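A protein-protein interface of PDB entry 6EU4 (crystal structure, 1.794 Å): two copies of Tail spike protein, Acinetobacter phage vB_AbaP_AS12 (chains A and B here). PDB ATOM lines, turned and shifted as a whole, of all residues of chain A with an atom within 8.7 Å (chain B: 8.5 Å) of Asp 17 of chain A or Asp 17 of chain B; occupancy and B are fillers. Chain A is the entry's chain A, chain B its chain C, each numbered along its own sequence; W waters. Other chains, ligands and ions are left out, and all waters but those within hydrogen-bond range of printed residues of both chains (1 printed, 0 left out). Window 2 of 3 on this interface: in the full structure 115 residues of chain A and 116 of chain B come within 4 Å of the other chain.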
ATOM      1  N   VAL A  16       5.792  -8.041 -20.230  1.00  0.00           N
ATOM      2  CA  VAL A  16       6.651  -8.762 -19.290  1.00  0.00           C
ATOM      3  C   VAL A  16       7.496  -9.813 -20.019  1.00  0.00           C
ATOM      4  O   VAL A  16       6.991 -10.594 -20.830  1.00  0.00           O
ATOM      5  CB  VAL A  16       5.822  -9.412 -18.170  1.00  0.00           C
ATOM      6  CG1 VAL A  16       4.957 -10.547 -18.722  1.00  0.00           C
ATOM      7  CG2 VAL A  16       6.735  -9.906 -17.050  1.00  0.00           C
ATOM      8  N   ASP A  17       8.785  -9.836 -19.702  1.00  0.00           N
ATOM      9  CA  ASP A  17       9.775 -10.602 -20.442  1.00  0.00           C
ATOM     10  C   ASP A  17      10.184 -11.849 -19.671  1.00  0.00           C
ATOM     11  O   ASP A  17       9.901 -11.999 -18.483  1.00  0.00           O
ATOM     12  CB  ASP A  17      11.010  -9.741 -20.720  1.00  0.00           C
ATOM     13  CG  ASP A  17      10.682  -8.474 -21.483  1.00  0.00           C
ATOM     14  OD1 ASP A  17       9.543  -8.358 -21.991  1.00  0.00           O
ATOM     15  OD2 ASP A  17      11.569  -7.593 -21.572  1.00  0.00           O
ATOM     16  N   VAL A  18      10.875 -12.746 -20.372  1.00  0.00           N
ATOM     17  CA  VAL A  18      11.454 -13.928 -19.749  1.00  0.00           C
ATOM     18  C   VAL A  18      12.711 -13.521 -18.993  1.00  0.00           C
ATOM     19  O   VAL A  18      13.627 -12.925 -19.572  1.00  0.00           O
ATOM     20  CB  VAL A  18      11.771 -15.001 -20.807  1.00  0.00           C
ATOM     21  CG1 VAL A  18      12.400 -16.215 -20.150  1.00  0.00           C
ATOM     22  CG2 VAL A  18      10.515 -15.384 -21.575  1.00  0.00           C
ATOM     23  N   LYS A  19      12.755 -13.846 -17.700  1.00  0.00           N
ATOM     24  CA  LYS A  19      13.872 -13.492 -16.833  1.00  0.00           C
ATOM     25  C   LYS A  19      14.923 -14.593 -16.856  1.00  0.00           C
ATOM     26  O   LYS A  19      14.590 -15.779 -16.822  1.00  0.00           O
ATOM     27  CB  LYS A  19      13.396 -13.276 -15.395  1.00  0.00           C
ATOM     28  CG  LYS A  19      14.539 -13.083 -14.395  1.00  0.00           C
ATOM     29  CD  LYS A  19      14.038 -12.697 -13.002  1.00  0.00           C
ATOM     30  CE  LYS A  19      15.158 -12.132 -12.117  1.00  0.00           C
ATOM     31  NZ  LYS A  19      15.978 -11.076 -12.795  1.00  0.00           N
ATOM     32  N   ILE A  20      16.199 -14.190 -16.891  1.00  0.00           N
ATOM     33  CA  ILE A  20      17.318 -15.128 -16.884  1.00  0.00           C
ATOM     34  C   ILE A  20      17.682 -15.460 -15.445  1.00  0.00           C
ATOM     35  O   ILE A  20      17.745 -14.581 -14.584  1.00  0.00           O
ATOM     36  CB  ILE A  20      18.535 -14.542 -17.624  1.00  0.00           C
ATOM     37  CG1 ILE A  20      18.236 -14.332 -19.107  1.00  0.00           C
ATOM     38  CG2 ILE A  20      19.753 -15.441 -17.463  1.00  0.00           C
ATOM     39  CD1 ILE A  20      19.259 -13.408 -19.780  1.00  0.00           C
ATOM     40  N   GLY A  35       2.903 -17.053 -12.133  1.00  0.00           N
ATOM     41  CA  GLY A  35       2.911 -17.154 -13.580  1.00  0.00           C
ATOM     42  C   GLY A  35       4.123 -16.574 -14.284  1.00  0.00           C
ATOM     43  O   GLY A  35       4.165 -16.600 -15.522  1.00  0.00           O
ATOM     44  N   MET A  36       5.093 -16.036 -13.550  1.00  0.00           N
ATOM     45  CA  MET A  36       6.334 -15.523 -14.127  1.00  0.00           C
ATOM     46  C   MET A  36       7.099 -16.636 -14.858  1.00  0.00           C
ATOM     47  O   MET A  36       7.065 -17.789 -14.438  1.00  0.00           O
ATOM     48  CB  MET A  36       7.194 -14.912 -13.009  1.00  0.00           C
ATOM     49  CG  MET A  36       8.535 -14.316 -13.433  1.00  0.00           C
ATOM     50  SD  MET A  36       9.388 -13.299 -11.972  1.00  0.00           S
ATOM     51  CE  MET A  36       8.160 -11.789 -11.901  1.00  0.00           C
ATOM     52  N   VAL A  37       7.800 -16.291 -15.941  1.00  0.00           N
ATOM     53  CA  VAL A  37       8.590 -17.254 -16.712  1.00  0.00           C
ATOM     54  C   VAL A  37      10.062 -16.887 -16.594  1.00  0.00           C
ATOM     55  O   VAL A  37      10.443 -15.730 -16.817  1.00  0.00           O
ATOM     56  CB  VAL A  37       8.174 -17.292 -18.194  1.00  0.00           C
ATOM     57  CG1 VAL A  37       8.981 -18.356 -18.944  1.00  0.00           C
ATOM     58  CG2 VAL A  37       6.675 -17.534 -18.345  1.00  0.00           C
ATOM     59  N   ALA A  38      10.887 -17.879 -16.263  1.00  0.00           N
ATOM     60  CA  ALA A  38      12.329 -17.734 -16.191  1.00  0.00           C
ATOM     61  C   ALA A  38      12.995 -18.750 -17.111  1.00  0.00           C
ATOM     62  O   ALA A  38      12.453 -19.828 -17.367  1.00  0.00           O
ATOM     63  CB  ALA A  38      12.839 -17.938 -14.758  1.00  0.00           C
ATOM     64  N   TYR A  39      14.177 -18.392 -17.599  1.00  0.00           N
ATOM     65  CA  TYR A  39      15.050 -19.302 -18.328  1.00  0.00           C
ATOM     66  C   TYR A  39      16.271 -19.580 -17.465  1.00  0.00           C
ATOM     67  O   TYR A  39      17.026 -18.658 -17.150  1.00  0.00           O
ATOM     68  CB  TYR A  39      15.471 -18.717 -19.674  1.00  0.00           C
ATOM     69  CG  TYR A  39      16.352 -19.655 -20.469  1.00  0.00           C
ATOM     70  CD1 TYR A  39      15.799 -20.695 -21.203  1.00  0.00           C
ATOM     71  CD2 TYR A  39      17.732 -19.513 -20.471  1.00  0.00           C
ATOM     72  CE1 TYR A  39      16.599 -21.569 -21.927  1.00  0.00           C
ATOM     73  CE2 TYR A  39      18.535 -20.367 -21.191  1.00  0.00           C
ATOM     74  CZ  TYR A  39      17.967 -21.394 -21.917  1.00  0.00           C
ATOM     75  OH  TYR A  39      18.773 -22.248 -22.626  1.00  0.00           O
ATOM     76  N   TRP A  80       8.834 -23.221  -8.919  1.00  0.00           N
ATOM     77  CA  TRP A  80       9.209 -23.023 -10.315  1.00  0.00           C
ATOM     78  C   TRP A  80       9.131 -24.363 -11.040  1.00  0.00           C
ATOM     79  O   TRP A  80       9.957 -25.259 -10.812  1.00  0.00           O
ATOM     80  CB  TRP A  80      10.603 -22.411 -10.407  1.00  0.00           C
ATOM     81  CG  TRP A  80      10.633 -20.987  -9.953  1.00  0.00           C
ATOM     82  CD1 TRP A  80      10.871 -20.536  -8.688  1.00  0.00           C
ATOM     83  CD2 TRP A  80      10.408 -19.825 -10.759  1.00  0.00           C
ATOM     84  NE1 TRP A  80      10.811 -19.168  -8.657  1.00  0.00           N
ATOM     85  CE2 TRP A  80      10.535 -18.703  -9.916  1.00  0.00           C
ATOM     86  CE3 TRP A  80      10.120 -19.622 -12.111  1.00  0.00           C
ATOM     87  CZ2 TRP A  80      10.362 -17.398 -10.373  1.00  0.00           C
ATOM     88  CZ3 TRP A  80       9.958 -18.315 -12.571  1.00  0.00           C
ATOM     89  CH2 TRP A  80      10.087 -17.223 -11.701  1.00  0.00           C
ATOM     90  N   VAL B  16      15.597  -5.908 -28.015  1.00  0.00           N
ATOM     91  CA  VAL B  16      14.223  -6.389 -27.907  1.00  0.00           C
ATOM     92  C   VAL B  16      14.211  -7.777 -27.281  1.00  0.00           C
ATOM     93  O   VAL B  16      15.067  -8.610 -27.582  1.00  0.00           O
ATOM     94  CB  VAL B  16      13.523  -6.406 -29.271  1.00  0.00           C
ATOM     95  CG1 VAL B  16      12.046  -6.751 -29.098  1.00  0.00           C
ATOM     96  CG2 VAL B  16      13.687  -5.062 -29.975  1.00  0.00           C
ATOM     97  N   ASP B  17      13.221  -8.030 -26.427  1.00  0.00           N
ATOM     98  CA  ASP B  17      13.217  -9.192 -25.555  1.00  0.00           C
ATOM     99  C   ASP B  17      12.031 -10.098 -25.854  1.00  0.00           C
ATOM    100  O   ASP B  17      11.058  -9.705 -26.502  1.00  0.00           O
ATOM    101  CB  ASP B  17      13.182  -8.767 -24.078  1.00  0.00           C
ATOM    102  CG  ASP B  17      14.363  -7.888 -23.696  1.00  0.00           C
ATOM    103  OD1 ASP B  17      15.421  -7.980 -24.359  1.00  0.00           O
ATOM    104  OD2 ASP B  17      14.236  -7.109 -22.731  1.00  0.00           O
ATOM    105  N   VAL B  18      12.125 -11.327 -25.363  1.00  0.00           N
ATOM    106  CA  VAL B  18      11.073 -12.312 -25.561  1.00  0.00           C
ATOM    107  C   VAL B  18       9.911 -12.004 -24.629  1.00  0.00           C
ATOM    108  O   VAL B  18      10.087 -11.887 -23.412  1.00  0.00           O
ATOM    109  CB  VAL B  18      11.607 -13.729 -25.321  1.00  0.00           C
ATOM    110  CG1 VAL B  18      10.492 -14.753 -25.530  1.00  0.00           C
ATOM    111  CG2 VAL B  18      12.801 -14.007 -26.247  1.00  0.00           C
ATOM    112  N   LYS B  19       8.718 -11.910 -25.200  1.00  0.00           N
ATOM    113  CA  LYS B  19       7.501 -11.536 -24.495  1.00  0.00           C
ATOM    114  C   LYS B  19       6.731 -12.783 -24.077  1.00  0.00           C
ATOM    115  O   LYS B  19       6.628 -13.745 -24.839  1.00  0.00           O
ATOM    116  CB  LYS B  19       6.644 -10.660 -25.409  1.00  0.00           C
ATOM    117  CG  LYS B  19       5.379 -10.062 -24.823  1.00  0.00           C
ATOM    118  CD  LYS B  19       4.817  -9.060 -25.848  1.00  0.00           C
ATOM    119  CE  LYS B  19       3.553  -8.367 -25.404  1.00  0.00           C
ATOM    120  NZ  LYS B  19       3.141  -7.351 -26.436  1.00  0.00           N
ATOM    121  N   ILE B  20       6.192 -12.761 -22.879  1.00  0.00           N
ATOM    122  CA  ILE B  20       5.438 -13.887 -22.350  1.00  0.00           C
ATOM    123  C   ILE B  20       3.980 -13.756 -22.766  1.00  0.00           C
ATOM    124  O   ILE B  20       3.386 -12.674 -22.683  1.00  0.00           O
ATOM    125  CB  ILE B  20       5.564 -13.960 -20.816  1.00  0.00           C
ATOM    126  CG1 ILE B  20       7.027 -14.154 -20.398  1.00  0.00           C
ATOM    127  CG2 ILE B  20       4.709 -15.096 -20.272  1.00  0.00           C
ATOM    128  CD1 ILE B  20       7.278 -13.853 -18.918  1.00  0.00           C
ATOM    129  N   VAL B  21       3.393 -14.877 -23.172  1.00  0.00           N
ATOM    130  CA  VAL B  21       1.976 -14.976 -23.496  1.00  0.00           C
ATOM    131  C   VAL B  21       1.421 -16.188 -22.758  1.00  0.00           C
ATOM    132  O   VAL B  21       2.051 -17.251 -22.743  1.00  0.00           O
ATOM    133  CB  VAL B  21       1.764 -15.109 -25.020  1.00  0.00           C
ATOM    134  CG1 VAL B  21       0.300 -15.323 -25.344  1.00  0.00           C
ATOM    135  CG2 VAL B  21       2.312 -13.876 -25.738  1.00  0.00           C
ATOM    136  N   GLY B  35       8.310  -9.990 -36.867  1.00  0.00           N
ATOM    137  CA  GLY B  35       9.513 -10.615 -36.349  1.00  0.00           C
ATOM    138  C   GLY B  35       9.595 -10.717 -34.839  1.00  0.00           C
ATOM    139  O   GLY B  35      10.575 -11.264 -34.325  1.00  0.00           O
ATOM    140  N   MET B  36       8.610 -10.197 -34.119  1.00  0.00           N
ATOM    141  CA  MET B  36       8.553 -10.300 -32.668  1.00  0.00           C
ATOM    142  C   MET B  36       8.565 -11.763 -32.217  1.00  0.00           C
ATOM    143  O   MET B  36       8.036 -12.626 -32.916  1.00  0.00           O
ATOM    144  CB  MET B  36       7.289  -9.591 -32.177  1.00  0.00           C
ATOM    145  CG  MET B  36       7.076  -9.558 -30.680  1.00  0.00           C
ATOM    146  SD  MET B  36       5.577  -8.377 -30.256  1.00  0.00           S
ATOM    147  CE  MET B  36       6.434  -6.672 -30.653  1.00  0.00           C
ATOM    148  N   VAL B  37       9.150 -12.032 -31.046  1.00  0.00           N
ATOM    149  CA  VAL B  37       9.228 -13.372 -30.469  1.00  0.00           C
ATOM    150  C   VAL B  37       8.445 -13.406 -29.165  1.00  0.00           C
ATOM    151  O   VAL B  37       8.623 -12.537 -28.300  1.00  0.00           O
ATOM    152  CB  VAL B  37      10.681 -13.809 -30.217  1.00  0.00           C
ATOM    153  CG1 VAL B  37      10.706 -15.242 -29.707  1.00  0.00           C
ATOM    154  CG2 VAL B  37      11.513 -13.679 -31.496  1.00  0.00           C
ATOM    155  N   ALA B  38       7.601 -14.424 -29.021  1.00  0.00           N
ATOM    156  CA  ALA B  38       6.820 -14.649 -27.816  1.00  0.00           C
ATOM    157  C   ALA B  38       7.062 -16.058 -27.300  1.00  0.00           C
ATOM    158  O   ALA B  38       7.323 -16.981 -28.075  1.00  0.00           O
ATOM    159  CB  ALA B  38       5.323 -14.469 -28.073  1.00  0.00           C
ATOM    160  N   TYR B  39       6.963 -16.224 -25.988  1.00  0.00           N
ATOM    161  CA  TYR B  39       6.982 -17.547 -25.371  1.00  0.00           C
ATOM    162  C   TYR B  39       5.597 -17.821 -24.800  1.00  0.00           C
ATOM    163  O   TYR B  39       5.160 -17.141 -23.869  1.00  0.00           O
ATOM    164  CB  TYR B  39       8.048 -17.649 -24.283  1.00  0.00           C
ATOM    165  CG  TYR B  39       8.083 -19.025 -23.656  1.00  0.00           C
ATOM    166  CD1 TYR B  39       8.795 -20.063 -24.246  1.00  0.00           C
ATOM    167  CD2 TYR B  39       7.389 -19.292 -22.488  1.00  0.00           C
ATOM    168  CE1 TYR B  39       8.821 -21.321 -23.685  1.00  0.00           C
ATOM    169  CE2 TYR B  39       7.403 -20.555 -21.926  1.00  0.00           C
ATOM    170  CZ  TYR B  39       8.123 -21.561 -22.524  1.00  0.00           C
ATOM    171  OH  TYR B  39       8.133 -22.813 -21.960  1.00  0.00           O
HETATM  172  O   HOH W   1      13.111 -11.643 -22.383  1.00  0.00           O
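Asp 17 of chain A touches just these residues of chain B: Asp 17, Val 18 and Ile 20.
Asp 17 of chain B touches one residue of chain A.
Printed residues of chain A within 4 Å of Tyr 39 of chain B: Val 37.
Of the printed residues of chain B, Val 18 of chain A touches Val 18 (3.3 Å) and Ile 20 (3.9 Å).
Printed residues of chain A within 4 Å of Lys 19 of chain B: Val 16.
Ala 38 of chain B touches none of the printed residues of chain A.
The nearest residue of chain A that does not touch Asp 17 of chain B is Val 18 of chain A (5.9 Å).
The nearest printed residue of chain A that does not touch Val 18 of chain B is Val 16 of chain A (4.2 Å).
O of Tyr 39 of chain B is in hydrogen-bond range of N of Val 21 of chain B, 3.0 Å away.
O of Val 37 of chain B sits at hydrogen-bond distance from N of Lys 19 of chain B.
O of Val 37 of chain A lies within hydrogen-bond range of N of Lys 19 of chain A (3.1 Å).
The backbone NH (N) of Tyr 39 of chain B lies within hydrogen-bond range of the backbone carbonyl oxygen (O) of Lys 19 of chain B.
The backbone NH (N) of Val 18 of chain A sits at hydrogen-bond distance from the backbone carbonyl oxygen (O) of Val 18 of chain B (3.3 Å).
N of Ile 20 of chain B lies within hydrogen-bond range of O of Val 16 of chain A (3.1 Å).
OD2 of Asp 17 of chain A sits close to OD2 of Asp 17 of chain B, 2.9 Å away.
Hydrophobic or aromatic side chains of chain A within 4 Å of the printed part of chain B: Val 18 and Val 37.
Printed residues of chain B that touch a printed residue of chain A: Asp 17, Val 18, Lys 19, Ile 20 and Tyr 39.
Hydrophobic or aromatic side chains of chain B within 4 Å of the printed part of chain A: Ile 20 and Tyr 39.
Among the printed residues, pairs that only touch across the chains: Asp 17 of chain A with Ile 20 of chain B (3.2 Å), Asp 17 of chain A with Val 18 of chain B (3.3 Å), Val 37 of chain A with Ile 20 of chain B (3.6 Å), Val 16 of chain A with Lys 19 of chain B (3.8 Å), Val 18 of chain A with Ile 20 of chain B (3.9 Å) and Val 37 of chain A with Tyr 39 of chain B (3.996 Å).
Val 16 of chain A touches Lys 19 of chain B, but with the chains exchanged Lys 19 of chain A does not touch Val 16 of chain B (11.4 Å).
Asp 17 of chain A touches Ile 20 of chain B, but with the chains exchanged Ile 20 of chain A does not touch Asp 17 of chain B (8.1 Å).
Val 18 of chain A touches its own counterpart, Val 18 of chain B.
Val 18 of chain A touches Ile 20 of chain B, but with the chains exchanged Ile 20 of chain A does not touch Val 18 of chain B (9.0 Å).
Positions printed for both chains: 16, 17, 18, 19, 20, 35, 36, 37, 38 and 39.
Of the 9 pairs that touch across the chains among the printed residues, 2 have their exchanged pair printed and touching as well.
Water W1 bridges the backbone carbonyl oxygen (O) of Val 18 of chain A and the backbone NH (N) of Val 18 of chain B.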
